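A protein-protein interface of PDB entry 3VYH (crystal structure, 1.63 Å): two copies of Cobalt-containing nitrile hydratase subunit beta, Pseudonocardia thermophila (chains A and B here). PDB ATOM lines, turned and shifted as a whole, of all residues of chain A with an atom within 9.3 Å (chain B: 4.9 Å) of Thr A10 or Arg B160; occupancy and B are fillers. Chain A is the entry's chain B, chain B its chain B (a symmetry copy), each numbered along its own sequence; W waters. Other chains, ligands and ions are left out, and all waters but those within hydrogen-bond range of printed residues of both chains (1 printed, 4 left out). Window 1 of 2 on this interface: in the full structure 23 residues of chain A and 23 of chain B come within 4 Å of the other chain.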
ATOM      1  N   ASN A   2      -6.384  21.202 -12.452  1.00  0.00           N
ATOM      2  CA  ASN A   2      -7.454  20.286 -12.066  1.00  0.00           C
ATOM      3  C   ASN A   2      -7.241  18.903 -12.693  1.00  0.00           C
ATOM      4  O   ASN A   2      -8.136  18.381 -13.347  1.00  0.00           O
ATOM      5  CB  ASN A   2      -8.863  20.789 -12.508  1.00  0.00           C
ATOM      6  CG  ASN A   2      -9.318  22.054 -11.820  1.00  0.00           C
ATOM      7  OD1 ASN A   2     -10.360  22.673 -12.250  1.00  0.00           O
ATOM      8  ND2 ASN A   2      -8.649  22.443 -10.801  1.00  0.00           N
ATOM      9  N   GLY A   3      -6.108  18.268 -12.399  1.00  0.00           N
ATOM     10  CA  GLY A   3      -5.782  17.009 -13.036  1.00  0.00           C
ATOM     11  C   GLY A   3      -6.460  15.840 -12.357  1.00  0.00           C
ATOM     12  O   GLY A   3      -6.787  15.872 -11.159  1.00  0.00           O
ATOM     13  N   VAL A   4      -6.525  14.727 -13.122  1.00  0.00           N
ATOM     14  CA  VAL A   4      -7.049  13.508 -12.557  1.00  0.00           C
ATOM     15  C   VAL A   4      -6.170  12.995 -11.408  1.00  0.00           C
ATOM     16  O   VAL A   4      -6.681  12.350 -10.524  1.00  0.00           O
ATOM     17  CB  VAL A   4      -7.220  12.432 -13.682  1.00  0.00           C
ATOM     18  CG1 VAL A   4      -7.615  11.096 -13.107  1.00  0.00           C
ATOM     19  CG2 VAL A   4      -8.299  12.936 -14.596  1.00  0.00           C
ATOM     20  N   TYR A   5      -4.877  13.332 -11.402  1.00  0.00           N
ATOM     21  CA  TYR A   5      -3.944  12.803 -10.423  1.00  0.00           C
ATOM     22  C   TYR A   5      -4.333  13.234  -9.005  1.00  0.00           C
ATOM     23  O   TYR A   5      -3.916  12.579  -8.036  1.00  0.00           O
ATOM     24  CB  TYR A   5      -2.495  13.416 -10.757  1.00  0.00           C
ATOM     25  CG  TYR A   5      -2.404  14.867 -10.227  1.00  0.00           C
ATOM     26  CD1 TYR A   5      -1.922  15.090  -8.895  1.00  0.00           C
ATOM     27  CD2 TYR A   5      -2.924  15.986 -10.986  1.00  0.00           C
ATOM     28  CE1 TYR A   5      -1.897  16.357  -8.325  1.00  0.00           C
ATOM     29  CE2 TYR A   5      -2.947  17.286 -10.364  1.00  0.00           C
ATOM     30  CZ  TYR A   5      -2.418  17.429  -9.069  1.00  0.00           C
ATOM     31  OH  TYR A   5      -2.397  18.722  -8.496  1.00  0.00           O
ATOM     32  N   ASP A   6      -5.130  14.317  -8.901  1.00  0.00           N
ATOM     33  CA  ASP A   6      -5.561  14.854  -7.536  1.00  0.00           C
ATOM     34  C   ASP A   6      -6.766  13.959  -7.180  1.00  0.00           C
ATOM     35  O   ASP A   6      -7.959  14.270  -7.495  1.00  0.00           O
ATOM     36  CB  ASP A   6      -5.887  16.340  -7.800  1.00  0.00           C
ATOM     37  CG  ASP A   6      -6.821  16.970  -6.773  1.00  0.00           C
ATOM     38  OD1 ASP A   6      -6.919  16.517  -5.644  1.00  0.00           O
ATOM     39  OD2 ASP A   6      -7.421  17.999  -7.188  1.00  0.00           O
ATOM     40  N   VAL A   7      -6.416  12.795  -6.591  1.00  0.00           N
ATOM     41  CA  VAL A   7      -7.427  11.751  -6.532  1.00  0.00           C
ATOM     42  C   VAL A   7      -8.161  11.725  -5.157  1.00  0.00           C
ATOM     43  O   VAL A   7      -9.096  10.905  -5.023  1.00  0.00           O
ATOM     44  CB  VAL A   7      -6.872  10.326  -6.755  1.00  0.00           C
ATOM     45  CG1 VAL A   7      -6.275  10.141  -8.131  1.00  0.00           C
ATOM     46  CG2 VAL A   7      -5.817   9.953  -5.628  1.00  0.00           C
ATOM     47  N   GLY A   8      -7.789  12.588  -4.205  1.00  0.00           N
ATOM     48  CA  GLY A   8      -8.480  12.439  -2.906  1.00  0.00           C
ATOM     49  C   GLY A   8      -9.972  12.670  -3.060  1.00  0.00           C
ATOM     50  O   GLY A   8     -10.459  13.667  -3.617  1.00  0.00           O
ATOM     51  N   GLY A   9     -10.714  11.716  -2.550  1.00  0.00           N
ATOM     52  CA  GLY A   9     -12.213  11.765  -2.609  1.00  0.00           C
ATOM     53  C   GLY A   9     -12.762  11.170  -3.934  1.00  0.00           C
ATOM     54  O   GLY A   9     -13.969  11.075  -4.061  1.00  0.00           O
ATOM     55  N   THR A  10     -11.930  10.838  -4.938  1.00  0.00           N
ATOM     56  CA  THR A  10     -12.486  10.187  -6.130  1.00  0.00           C
ATOM     57  C   THR A  10     -13.032   8.787  -5.734  1.00  0.00           C
ATOM     58  O   THR A  10     -12.349   8.015  -5.012  1.00  0.00           O
ATOM     59  CB  THR A  10     -11.351  10.049  -7.133  1.00  0.00           C
ATOM     60  OG1 THR A  10     -11.022  11.343  -7.586  1.00  0.00           O
ATOM     61  CG2 THR A  10     -11.864   9.250  -8.368  1.00  0.00           C
ATOM     62  N   ASP A  11     -14.260   8.482  -6.188  1.00  0.00           N
ATOM     63  CA  ASP A  11     -14.871   7.158  -6.087  1.00  0.00           C
ATOM     64  C   ASP A  11     -14.599   6.292  -7.335  1.00  0.00           C
ATOM     65  O   ASP A  11     -14.361   6.800  -8.396  1.00  0.00           O
ATOM     66  CB  ASP A  11     -16.374   7.308  -5.954  1.00  0.00           C
ATOM     67  CG  ASP A  11     -16.796   7.962  -4.639  1.00  0.00           C
ATOM     68  OD1 ASP A  11     -16.152   7.666  -3.599  1.00  0.00           O
ATOM     69  OD2 ASP A  11     -17.826   8.745  -4.624  1.00  0.00           O
ATOM     70  N   GLY A  12     -14.709   4.976  -7.106  1.00  0.00           N
ATOM     71  CA  GLY A  12     -14.699   4.084  -8.303  1.00  0.00           C
ATOM     72  C   GLY A  12     -13.355   3.561  -8.743  1.00  0.00           C
ATOM     73  O   GLY A  12     -13.302   2.840  -9.742  1.00  0.00           O
ATOM     74  N   LEU A  13     -12.289   3.883  -7.993  1.00  0.00           N
ATOM     75  CA  LEU A  13     -10.946   3.426  -8.363  1.00  0.00           C
ATOM     76  C   LEU A  13     -10.613   1.997  -8.021  1.00  0.00           C
ATOM     77  O   LEU A  13      -9.627   1.478  -8.531  1.00  0.00           O
ATOM     78  CB  LEU A  13      -9.846   4.372  -7.824  1.00  0.00           C
ATOM     79  CG  LEU A  13      -9.685   5.583  -8.705  1.00  0.00           C
ATOM     80  CD1 LEU A  13     -10.646   6.012  -9.777  1.00  0.00           C
ATOM     81  CD2 LEU A  13      -9.052   6.725  -7.957  1.00  0.00           C
ATOM     82  N   GLY A  14     -11.448   1.365  -7.234  1.00  0.00           N
ATOM     83  CA  GLY A  14     -11.388  -0.105  -7.009  1.00  0.00           C
ATOM     84  C   GLY A  14     -10.569  -0.438  -5.759  1.00  0.00           C
ATOM     85  O   GLY A  14     -10.119   0.442  -5.000  1.00  0.00           O
ATOM     86  N   LEU A  64      -2.950   6.449 -14.312  1.00  0.00           N
ATOM     87  CA  LEU A  64      -3.693   5.646 -13.349  1.00  0.00           C
ATOM     88  C   LEU A  64      -3.226   4.193 -13.336  1.00  0.00           C
ATOM     89  O   LEU A  64      -3.459   3.544 -12.333  1.00  0.00           O
ATOM     90  CB  LEU A  64      -5.219   5.678 -13.712  1.00  0.00           C
ATOM     91  CG  LEU A  64      -5.915   7.043 -13.364  1.00  0.00           C
ATOM     92  CD1 LEU A  64      -7.391   7.032 -13.851  1.00  0.00           C
ATOM     93  CD2 LEU A  64      -5.937   7.268 -11.824  1.00  0.00           C
ATOM     94  N   ARG A 160      -8.715  19.480  -5.132  1.00  0.00           N
ATOM     95  CA  ARG A 160     -10.129  19.928  -5.368  1.00  0.00           C
ATOM     96  C   ARG A 160     -11.040  19.650  -4.149  1.00  0.00           C
ATOM     97  O   ARG A 160     -11.913  20.476  -3.860  1.00  0.00           O
ATOM     98  CB  ARG A 160     -10.657  19.248  -6.674  1.00  0.00           C
ATOM     99  CG  ARG A 160     -10.251  20.007  -7.934  1.00  0.00           C
ATOM    100  CD  ARG A 160     -10.647  19.053  -9.247  1.00  0.00           C
ATOM    101  NE  ARG A 160     -10.047  17.711  -9.002  1.00  0.00           N
ATOM    102  CZ  ARG A 160     -10.200  16.602  -9.767  1.00  0.00           C
ATOM    103  NH1 ARG A 160     -10.911  16.682 -10.914  1.00  0.00           N
ATOM    104  NH2 ARG A 160      -9.641  15.417  -9.369  1.00  0.00           N
ATOM    105  N   TYR A 161     -10.777  18.585  -3.377  1.00  0.00           N
ATOM    106  CA  TYR A 161     -11.661  18.241  -2.249  1.00  0.00           C
ATOM    107  C   TYR A 161     -11.707  19.229  -1.111  1.00  0.00           C
ATOM    108  O   TYR A 161     -12.637  19.166  -0.319  1.00  0.00           O
ATOM    109  CB  TYR A 161     -11.462  16.800  -1.714  1.00  0.00           C
ATOM    110  CG  TYR A 161     -10.294  16.534  -0.838  1.00  0.00           C
ATOM    111  CD1 TYR A 161      -9.012  16.242  -1.360  1.00  0.00           C
ATOM    112  CD2 TYR A 161     -10.465  16.575   0.562  1.00  0.00           C
ATOM    113  CE1 TYR A 161      -7.901  15.964  -0.497  1.00  0.00           C
ATOM    114  CE2 TYR A 161      -9.347  16.279   1.394  1.00  0.00           C
ATOM    115  CZ  TYR A 161      -8.100  16.021   0.886  1.00  0.00           C
ATOM    116  OH  TYR A 161      -7.098  15.785   1.801  1.00  0.00           O
ATOM    117  N   ARG A 163     -11.159  22.738  -1.678  1.00  0.00           N
ATOM    118  CA  ARG A 163     -11.389  24.110  -2.167  1.00  0.00           C
ATOM    119  C   ARG A 163     -12.777  24.584  -1.710  1.00  0.00           C
ATOM    120  O   ARG A 163     -13.776  23.851  -1.840  1.00  0.00           O
ATOM    121  CB  ARG A 163     -11.356  24.147  -3.684  1.00  0.00           C
ATOM    122  CG  ARG A 163      -9.896  23.799  -4.201  1.00  0.00           C
ATOM    123  CD  ARG A 163      -9.815  24.095  -5.691  1.00  0.00           C
ATOM    124  NE  ARG A 163      -8.691  23.393  -6.276  1.00  0.00           N
ATOM    125  CZ  ARG A 163      -8.518  23.245  -7.566  1.00  0.00           C
ATOM    126  NH1 ARG A 163      -9.412  23.759  -8.416  1.00  0.00           N
ATOM    127  NH2 ARG A 163      -7.487  22.511  -8.017  1.00  0.00           N
ATOM    128  N   LYS A 165     -13.829  24.913   1.192  1.00  0.00           N
ATOM    129  CA  LYS A 165     -14.234  24.338   2.478  1.00  0.00           C
ATOM    130  C   LYS A 165     -13.655  25.158   3.617  1.00  0.00           C
ATOM    131  O   LYS A 165     -12.595  25.774   3.519  1.00  0.00           O
ATOM    132  CB  LYS A 165     -13.682  22.926   2.597  1.00  0.00           C
ATOM    133  CG  LYS A 165     -14.317  21.969   1.513  1.00  0.00           C
ATOM    134  CD  LYS A 165     -15.928  21.964   1.470  1.00  0.00           C
ATOM    135  CE  LYS A 165     -16.560  20.803   0.630  1.00  0.00           C
ATOM    136  NZ  LYS A 165     -16.391  20.996  -0.868  1.00  0.00           N
ATOM    137  N   LEU A 203     -16.130  18.209   4.451  1.00  0.00           N
ATOM    138  CA  LEU A 203     -15.582  17.791   3.163  1.00  0.00           C
ATOM    139  C   LEU A 203     -16.596  17.034   2.367  1.00  0.00           C
ATOM    140  O   LEU A 203     -16.651  17.270   1.117  1.00  0.00           O
ATOM    141  CB  LEU A 203     -14.329  16.936   3.400  1.00  0.00           C
ATOM    142  CG  LEU A 203     -13.126  17.647   4.018  1.00  0.00           C
ATOM    143  CD1 LEU A 203     -12.002  16.541   4.184  1.00  0.00           C
ATOM    144  CD2 LEU A 203     -12.694  18.864   3.226  1.00  0.00           C
ATOM    145  N   TRP A 204     -17.358  16.103   3.009  1.00  0.00           N
ATOM    146  CA  TRP A 204     -18.177  15.099   2.263  1.00  0.00           C
ATOM    147  C   TRP A 204     -19.689  15.274   2.430  1.00  0.00           C
ATOM    148  O   TRP A 204     -20.468  14.560   1.837  1.00  0.00           O
ATOM    149  CB  TRP A 204     -17.755  13.671   2.657  1.00  0.00           C
ATOM    150  CG  TRP A 204     -16.235  13.515   2.635  1.00  0.00           C
ATOM    151  CD1 TRP A 204     -15.438  13.164   3.714  1.00  0.00           C
ATOM    152  CD2 TRP A 204     -15.331  13.703   1.509  1.00  0.00           C
ATOM    153  NE1 TRP A 204     -14.118  13.127   3.339  1.00  0.00           N
ATOM    154  CE2 TRP A 204     -14.026  13.466   2.014  1.00  0.00           C
ATOM    155  CE3 TRP A 204     -15.501  14.060   0.149  1.00  0.00           C
ATOM    156  CZ2 TRP A 204     -12.880  13.512   1.215  1.00  0.00           C
ATOM    157  CZ3 TRP A 204     -14.309  14.168  -0.661  1.00  0.00           C
ATOM    158  CH2 TRP A 204     -13.032  13.941  -0.065  1.00  0.00           C
ATOM    159  N   ASN B   2     -18.386  10.170  -6.838  1.00  0.00           N
ATOM    160  CA  ASN B   2     -17.302  11.059  -7.247  1.00  0.00           C
ATOM    161  C   ASN B   2     -16.421  10.392  -8.310  1.00  0.00           C
ATOM    162  O   ASN B   2     -15.209  10.320  -8.145  1.00  0.00           O
ATOM    163  CB  ASN B   2     -16.376  11.463  -6.058  1.00  0.00           C
ATOM    164  CG  ASN B   2     -17.049  12.311  -5.004  1.00  0.00           C
ATOM    165  OD1 ASN B   2     -16.452  12.527  -3.886  1.00  0.00           O
ATOM    166  ND2 ASN B   2     -18.191  12.810  -5.291  1.00  0.00           N
ATOM    167  N   GLY B   3     -17.012  10.012  -9.441  1.00  0.00           N
ATOM    168  CA  GLY B   3     -16.274   9.277 -10.447  1.00  0.00           C
ATOM    169  C   GLY B   3     -15.461  10.194 -11.334  1.00  0.00           C
ATOM    170  O   GLY B   3     -15.784  11.378 -11.530  1.00  0.00           O
ATOM    171  N   VAL B   4     -14.467   9.566 -12.004  1.00  0.00           N
ATOM    172  CA  VAL B   4     -13.687  10.304 -12.966  1.00  0.00           C
ATOM    173  C   VAL B   4     -14.547  10.781 -14.144  1.00  0.00           C
ATOM    174  O   VAL B   4     -14.229  11.789 -14.729  1.00  0.00           O
ATOM    175  CB  VAL B   4     -12.477   9.432 -13.446  1.00  0.00           C
ATOM    176  CG1 VAL B   4     -11.728  10.106 -14.567  1.00  0.00           C
ATOM    177  CG2 VAL B   4     -11.575   9.261 -12.258  1.00  0.00           C
ATOM    178  N   ASP B   6     -17.126  12.344 -14.273  1.00  0.00           N
ATOM    179  CA  ASP B   6     -17.723  13.733 -14.050  1.00  0.00           C
ATOM    180  C   ASP B   6     -16.540  14.671 -14.371  1.00  0.00           C
ATOM    181  O   ASP B   6     -15.722  15.060 -13.479  1.00  0.00           O
ATOM    182  CB  ASP B   6     -18.181  13.717 -12.575  1.00  0.00           C
ATOM    183  CG  ASP B   6     -18.320  15.098 -11.945  1.00  0.00           C
ATOM    184  OD1 ASP B   6     -18.510  16.090 -12.629  1.00  0.00           O
ATOM    185  OD2 ASP B   6     -18.267  15.094 -10.684  1.00  0.00           O
ATOM    186  N   THR B  10     -12.182  19.302 -15.369  1.00  0.00           N
ATOM    187  CA  THR B  10     -10.900  18.591 -15.299  1.00  0.00           C
ATOM    188  C   THR B  10      -9.929  19.195 -16.352  1.00  0.00           C
ATOM    189  O   THR B  10     -10.318  19.415 -17.529  1.00  0.00           O
ATOM    190  CB  THR B  10     -11.181  17.130 -15.614  1.00  0.00           C
ATOM    191  OG1 THR B  10     -11.916  16.594 -14.536  1.00  0.00           O
ATOM    192  CG2 THR B  10      -9.830  16.358 -15.675  1.00  0.00           C
ATOM    193  N   ARG B 158     -24.708  15.361  -9.576  1.00  0.00           N
ATOM    194  CA  ARG B 158     -24.116  16.456  -8.723  1.00  0.00           C
ATOM    195  C   ARG B 158     -22.648  16.673  -9.156  1.00  0.00           C
ATOM    196  O   ARG B 158     -21.742  16.182  -8.475  1.00  0.00           O
ATOM    197  CB  ARG B 158     -24.177  16.100  -7.227  1.00  0.00           C
ATOM    198  CG  ARG B 158     -25.615  15.813  -6.714  1.00  0.00           C
ATOM    199  CD  ARG B 158     -25.538  14.999  -5.412  1.00  0.00           C
ATOM    200  NE  ARG B 158     -26.896  14.784  -4.876  1.00  0.00           N
ATOM    201  CZ  ARG B 158     -27.411  15.465  -3.853  1.00  0.00           C
ATOM    202  NH1 ARG B 158     -26.781  16.510  -3.349  1.00  0.00           N
ATOM    203  NH2 ARG B 158     -28.634  15.186  -3.467  1.00  0.00           N
ATOM    204  N   ALA B 159     -22.468  17.262 -10.322  1.00  0.00           N
ATOM    205  CA  ALA B 159     -21.102  17.489 -10.818  1.00  0.00           C
ATOM    206  C   ALA B 159     -20.254  18.100  -9.731  1.00  0.00           C
ATOM    207  O   ALA B 159     -20.635  19.106  -9.086  1.00  0.00           O
ATOM    208  CB  ALA B 159     -21.079  18.388 -12.074  1.00  0.00           C
ATOM    209  N   ARG B 160     -19.074  17.549  -9.496  1.00  0.00           N
ATOM    210  CA  ARG B 160     -18.207  18.128  -8.414  1.00  0.00           C
ATOM    211  C   ARG B 160     -17.955  19.641  -8.614  1.00  0.00           C
ATOM    212  O   ARG B 160     -17.913  20.373  -7.620  1.00  0.00           O
ATOM    213  CB  ARG B 160     -16.878  17.306  -8.345  1.00  0.00           C
ATOM    214  CG  ARG B 160     -17.015  16.042  -7.502  1.00  0.00           C
ATOM    215  CD  ARG B 160     -15.627  15.138  -7.720  1.00  0.00           C
ATOM    216  NE  ARG B 160     -15.433  14.993  -9.191  1.00  0.00           N
ATOM    217  CZ  ARG B 160     -14.379  14.414  -9.818  1.00  0.00           C
ATOM    218  NH1 ARG B 160     -13.404  13.839  -9.079  1.00  0.00           N
ATOM    219  NH2 ARG B 160     -14.311  14.422 -11.186  1.00  0.00           N
ATOM    220  N   TYR B 161     -17.909  20.126  -9.865  1.00  0.00           N
ATOM    221  CA  TYR B 161     -17.600  21.547 -10.105  1.00  0.00           C
ATOM    222  C   TYR B 161     -18.613  22.546  -9.606  1.00  0.00           C
ATOM    223  O   TYR B 161     -18.273  23.715  -9.486  1.00  0.00           O
ATOM    224  CB  TYR B 161     -17.197  21.862 -11.568  1.00  0.00           C
ATOM    225  CG  TYR B 161     -18.275  21.958 -12.584  1.00  0.00           C
ATOM    226  CD1 TYR B 161     -18.793  20.818 -13.243  1.00  0.00           C
ATOM    227  CD2 TYR B 161     -18.802  23.226 -12.905  1.00  0.00           C
ATOM    228  CE1 TYR B 161     -19.817  20.933 -14.240  1.00  0.00           C
ATOM    229  CE2 TYR B 161     -19.808  23.312 -13.910  1.00  0.00           C
ATOM    230  CZ  TYR B 161     -20.326  22.203 -14.529  1.00  0.00           C
ATOM    231  OH  TYR B 161     -21.319  22.423 -15.458  1.00  0.00           O
ATOM    232  N   VAL B 162     -19.829  22.066  -9.418  1.00  0.00           N
ATOM    233  CA  VAL B 162     -20.903  22.981  -8.890  1.00  0.00           C
ATOM    234  C   VAL B 162     -21.140  22.870  -7.394  1.00  0.00           C
ATOM    235  O   VAL B 162     -21.798  23.746  -6.792  1.00  0.00           O
ATOM    236  CB  VAL B 162     -22.252  22.877  -9.671  1.00  0.00           C
ATOM    237  CG1 VAL B 162     -22.084  23.328 -11.186  1.00  0.00           C
ATOM    238  CG2 VAL B 162     -22.974  21.516  -9.489  1.00  0.00           C
ATOM    239  N   ARG B 163     -20.655  21.836  -6.731  1.00  0.00           N
ATOM    240  CA  ARG B 163     -21.019  21.576  -5.326  1.00  0.00           C
ATOM    241  C   ARG B 163     -20.494  22.722  -4.447  1.00  0.00           C
ATOM    242  O   ARG B 163     -19.329  23.143  -4.575  1.00  0.00           O
ATOM    243  CB  ARG B 163     -20.383  20.285  -4.842  1.00  0.00           C
ATOM    244  CG  ARG B 163     -20.999  19.052  -5.629  1.00  0.00           C
ATOM    245  CD  ARG B 163     -20.549  17.762  -4.957  1.00  0.00           C
ATOM    246  NE  ARG B 163     -20.704  16.648  -5.869  1.00  0.00           N
ATOM    247  CZ  ARG B 163     -20.169  15.468  -5.673  1.00  0.00           C
ATOM    248  NH1 ARG B 163     -19.433  15.250  -4.580  1.00  0.00           N
ATOM    249  NH2 ARG B 163     -20.300  14.516  -6.613  1.00  0.00           N
HETATM  250  O   HOH W   1     -13.913   6.798 -11.158  1.00  0.00           O
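OD1 of Asn B2 sits close to O of Gly A9 (2.9 Å).
The side-chain carboxylate (OD2) of Asp A11 lies within hydrogen-bond range of the backbone NH (N) of Asn B2.
ND2 of Asn A2 lies close to NH1 of Arg A163 (2.8 Å).
The backbone carbonyl oxygen (O) of Gly A3 sits at hydrogen-bond distance from the guanidinium group (NH2) of Arg A160, at 3.4 Å.
The side-chain carboxylate (OD2) of Asp A6 lies within salt-bridge range of the guanidinium group (NE) of Arg A160, at 3.2 Å.
The side-chain hydroxyl of Thr A10 lies close to the backbone carbonyl oxygen of Val A7 (3.2 Å).
The side-chain amide nitrogen (ND2) of Asn B2 lies close to the guanidinium group (NH1) of Arg B163, 2.8 Å away.
NH2 of Arg B160 lies within hydrogen-bond range of O of Gly B3.
Among the printed residues, merely in contact across the chains: Thr A10 with Asn B2 (3.4 Å), Asn A2 with Thr B10 (3.4 Å), Asp A11 with Gly B3 (3.7 Å), Thr A10 with Arg B160 (3.8 Å), Arg A160 with Thr B10 (3.8 Å), Thr A10 with Val B4 (3.9 Å) and Val A4 with Thr B10 (3.9 Å).
Of the printed residues of chain B, Asn A2 touches Thr B10.
Printed residues of chain B within 4 Å of Gly A9: Asn B2 (2.9 Å).
Leu A13 touches none of the printed residues of chain B.
Gly A14 touches none of the printed residues of chain B.
Of the printed residues of chain B, Arg A160 touches Thr B10.
Gly B3 touches one residue of chain A.
Of the printed residues of chain A, Val B4 touches Thr A10.
No residue of chain A comes within 4 Å of Asp B6.
Printed residues of chain A within 4 Å of Arg B160: Thr A10.
Of the 20 printed residues of chain A, 6 touch a printed residue of chain B.
Among the printed residues, 9 pairs touch across the chains.
Asn A2 touches Thr B10, and with the chains exchanged Thr A10 touches Asn B2.
Val A4 touches Thr B10, and with the chains exchanged Thr A10 touches Val B4.
Thr A10 touches Arg B160, and with the chains exchanged Arg A160 touches Thr B10.
Positions printed for both chains: 2, 3, 4, 6, 10, 160, 161 and 163.
Water W1 bridges the backbone carbonyl oxygen of Asp A11 (2.8 Å) and the backbone NH of Val B4 (2.9 Å).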
